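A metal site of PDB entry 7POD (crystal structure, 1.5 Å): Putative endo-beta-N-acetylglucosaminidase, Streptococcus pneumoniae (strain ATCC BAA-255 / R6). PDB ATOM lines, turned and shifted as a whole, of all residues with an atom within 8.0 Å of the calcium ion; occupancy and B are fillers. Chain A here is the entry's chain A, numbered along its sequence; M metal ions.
OD1 of Asp 16 sits at hydrogen-bond distance from N of Gly 19 (3.2 Å).
The calcium ion is bound by OE1 of Glu 20, OD2 of Asp 16 and OD2 of Asp 18.
The calcium ion has three donor atoms within binding distance.
Three residues have an atom within 4 Å of the calcium ion: Asp 16, Asp 18 and Glu 20.
The nearest printed residue that does not touch the calcium ion is Leu 22 (6.1 Å).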
ATOM      1  N   TYR A  15      26.445  15.184 -29.054  1.00  0.00           N
ATOM      2  CA  TYR A  15      27.371  15.558 -27.978  1.00  0.00           C
ATOM      3  C   TYR A  15      28.698  14.814 -28.085  1.00  0.00           C
ATOM      4  O   TYR A  15      28.756  13.691 -28.618  1.00  0.00           O
ATOM      5  CB  TYR A  15      26.739  15.289 -26.612  1.00  0.00           C
ATOM      6  CG  TYR A  15      25.412  15.977 -26.396  1.00  0.00           C
ATOM      7  CD1 TYR A  15      25.368  17.258 -25.864  1.00  0.00           C
ATOM      8  CD2 TYR A  15      24.208  15.375 -26.693  1.00  0.00           C
ATOM      9  CE1 TYR A  15      24.163  17.891 -25.594  1.00  0.00           C
ATOM     10  CE2 TYR A  15      22.992  15.979 -26.456  1.00  0.00           C
ATOM     11  CZ  TYR A  15      22.969  17.254 -25.900  1.00  0.00           C
ATOM     12  OH  TYR A  15      21.775  17.866 -25.714  1.00  0.00           O
ATOM     13  N   ASP A  16      29.724  15.399 -27.479  1.00  0.00           N
ATOM     14  CA  ASP A  16      31.000  14.673 -27.278  1.00  0.00           C
ATOM     15  C   ASP A  16      30.956  13.899 -25.978  1.00  0.00           C
ATOM     16  O   ASP A  16      29.922  13.905 -25.274  1.00  0.00           O
ATOM     17  CB  ASP A  16      32.173  15.637 -27.400  1.00  0.00           C
ATOM     18  CG  ASP A  16      32.454  16.579 -26.258  1.00  0.00           C
ATOM     19  OD1 ASP A  16      31.744  16.549 -25.219  1.00  0.00           O
ATOM     20  OD2 ASP A  16      33.445  17.362 -26.427  1.00  0.00           O
ATOM     21  N   SER A  17      32.065  13.275 -25.609  1.00  0.00           N
ATOM     22  CA  SER A  17      32.086  12.424 -24.386  1.00  0.00           C
ATOM     23  C   SER A  17      31.988  13.273 -23.107  1.00  0.00           C
ATOM     24  O   SER A  17      31.667  12.692 -22.042  1.00  0.00           O
ATOM     25  CB  SER A  17      33.325  11.563 -24.379  1.00  0.00           C
ATOM     26  OG  SER A  17      34.486  12.372 -24.397  1.00  0.00           O
ATOM     27  N   ASP A  18      32.308  14.574 -23.168  1.00  0.00           N
ATOM     28  CA  ASP A  18      32.259  15.548 -22.036  1.00  0.00           C
ATOM     29  C   ASP A  18      30.823  16.081 -21.877  1.00  0.00           C
ATOM     30  O   ASP A  18      30.592  16.945 -20.977  1.00  0.00           O
ATOM     31  CB  ASP A  18      33.157  16.769 -22.272  1.00  0.00           C
ATOM     32  CG  ASP A  18      34.634  16.483 -22.492  1.00  0.00           C
ATOM     33  OD1 ASP A  18      35.130  15.593 -21.782  1.00  0.00           O
ATOM     34  OD2 ASP A  18      35.262  17.160 -23.420  1.00  0.00           O
ATOM     35  N   GLY A  19      29.916  15.717 -22.787  1.00  0.00           N
ATOM     36  CA  GLY A  19      28.573  16.308 -22.852  1.00  0.00           C
ATOM     37  C   GLY A  19      28.500  17.683 -23.508  1.00  0.00           C
ATOM     38  O   GLY A  19      27.433  18.333 -23.376  1.00  0.00           O
ATOM     39  N   GLU A  20      29.546  18.147 -24.179  1.00  0.00           N
ATOM     40  CA  GLU A  20      29.511  19.394 -24.971  1.00  0.00           C
ATOM     41  C   GLU A  20      28.798  19.165 -26.290  1.00  0.00           C
ATOM     42  O   GLU A  20      28.982  18.099 -26.945  1.00  0.00           O
ATOM     43  CB  GLU A  20      30.909  19.980 -25.161  1.00  0.00           C
ATOM     44  CG  GLU A  20      31.442  20.507 -23.830  1.00  0.00           C
ATOM     45  CD  GLU A  20      32.863  20.988 -23.931  1.00  0.00           C
ATOM     46  OE1 GLU A  20      33.734  20.173 -24.333  1.00  0.00           O
ATOM     47  OE2 GLU A  20      33.082  22.177 -23.663  1.00  0.00           O
ATOM     48  N   LYS A  21      27.972  20.128 -26.690  1.00  0.00           N
ATOM     49  CA  LYS A  21      27.269  20.049 -28.005  1.00  0.00           C
ATOM     50  C   LYS A  21      28.290  20.184 -29.146  1.00  0.00           C
ATOM     51  O   LYS A  21      29.068  21.145 -29.140  1.00  0.00           O
ATOM     52  CB  LYS A  21      26.200  21.140 -28.072  1.00  0.00           C
ATOM     53  CG  LYS A  21      25.161  21.044 -26.979  1.00  0.00           C
ATOM     54  CD  LYS A  21      24.250  22.257 -26.910  1.00  0.00           C
ATOM     55  CE  LYS A  21      23.878  22.630 -25.492  1.00  0.00           C
ATOM     56  NZ  LYS A  21      22.930  23.767 -25.466  1.00  0.00           N
ATOM     57  N   LEU A  22      28.255  19.241 -30.068  1.00  0.00           N
ATOM     58  CA  LEU A  22      29.060  19.277 -31.329  1.00  0.00           C
ATOM     59  C   LEU A  22      28.248  19.794 -32.513  1.00  0.00           C
ATOM     60  O   LEU A  22      28.787  20.538 -33.337  1.00  0.00           O
ATOM     61  CB  LEU A  22      29.555  17.869 -31.624  1.00  0.00           C
ATOM     62  CG  LEU A  22      30.520  17.310 -30.582  1.00  0.00           C
ATOM     63  CD1 LEU A  22      30.903  15.914 -30.972  1.00  0.00           C
ATOM     64  CD2 LEU A  22      31.755  18.171 -30.449  1.00  0.00           C
HETATM   65 CA    CA M   1      35.060  18.705 -25.391  1.00  0.00          CA
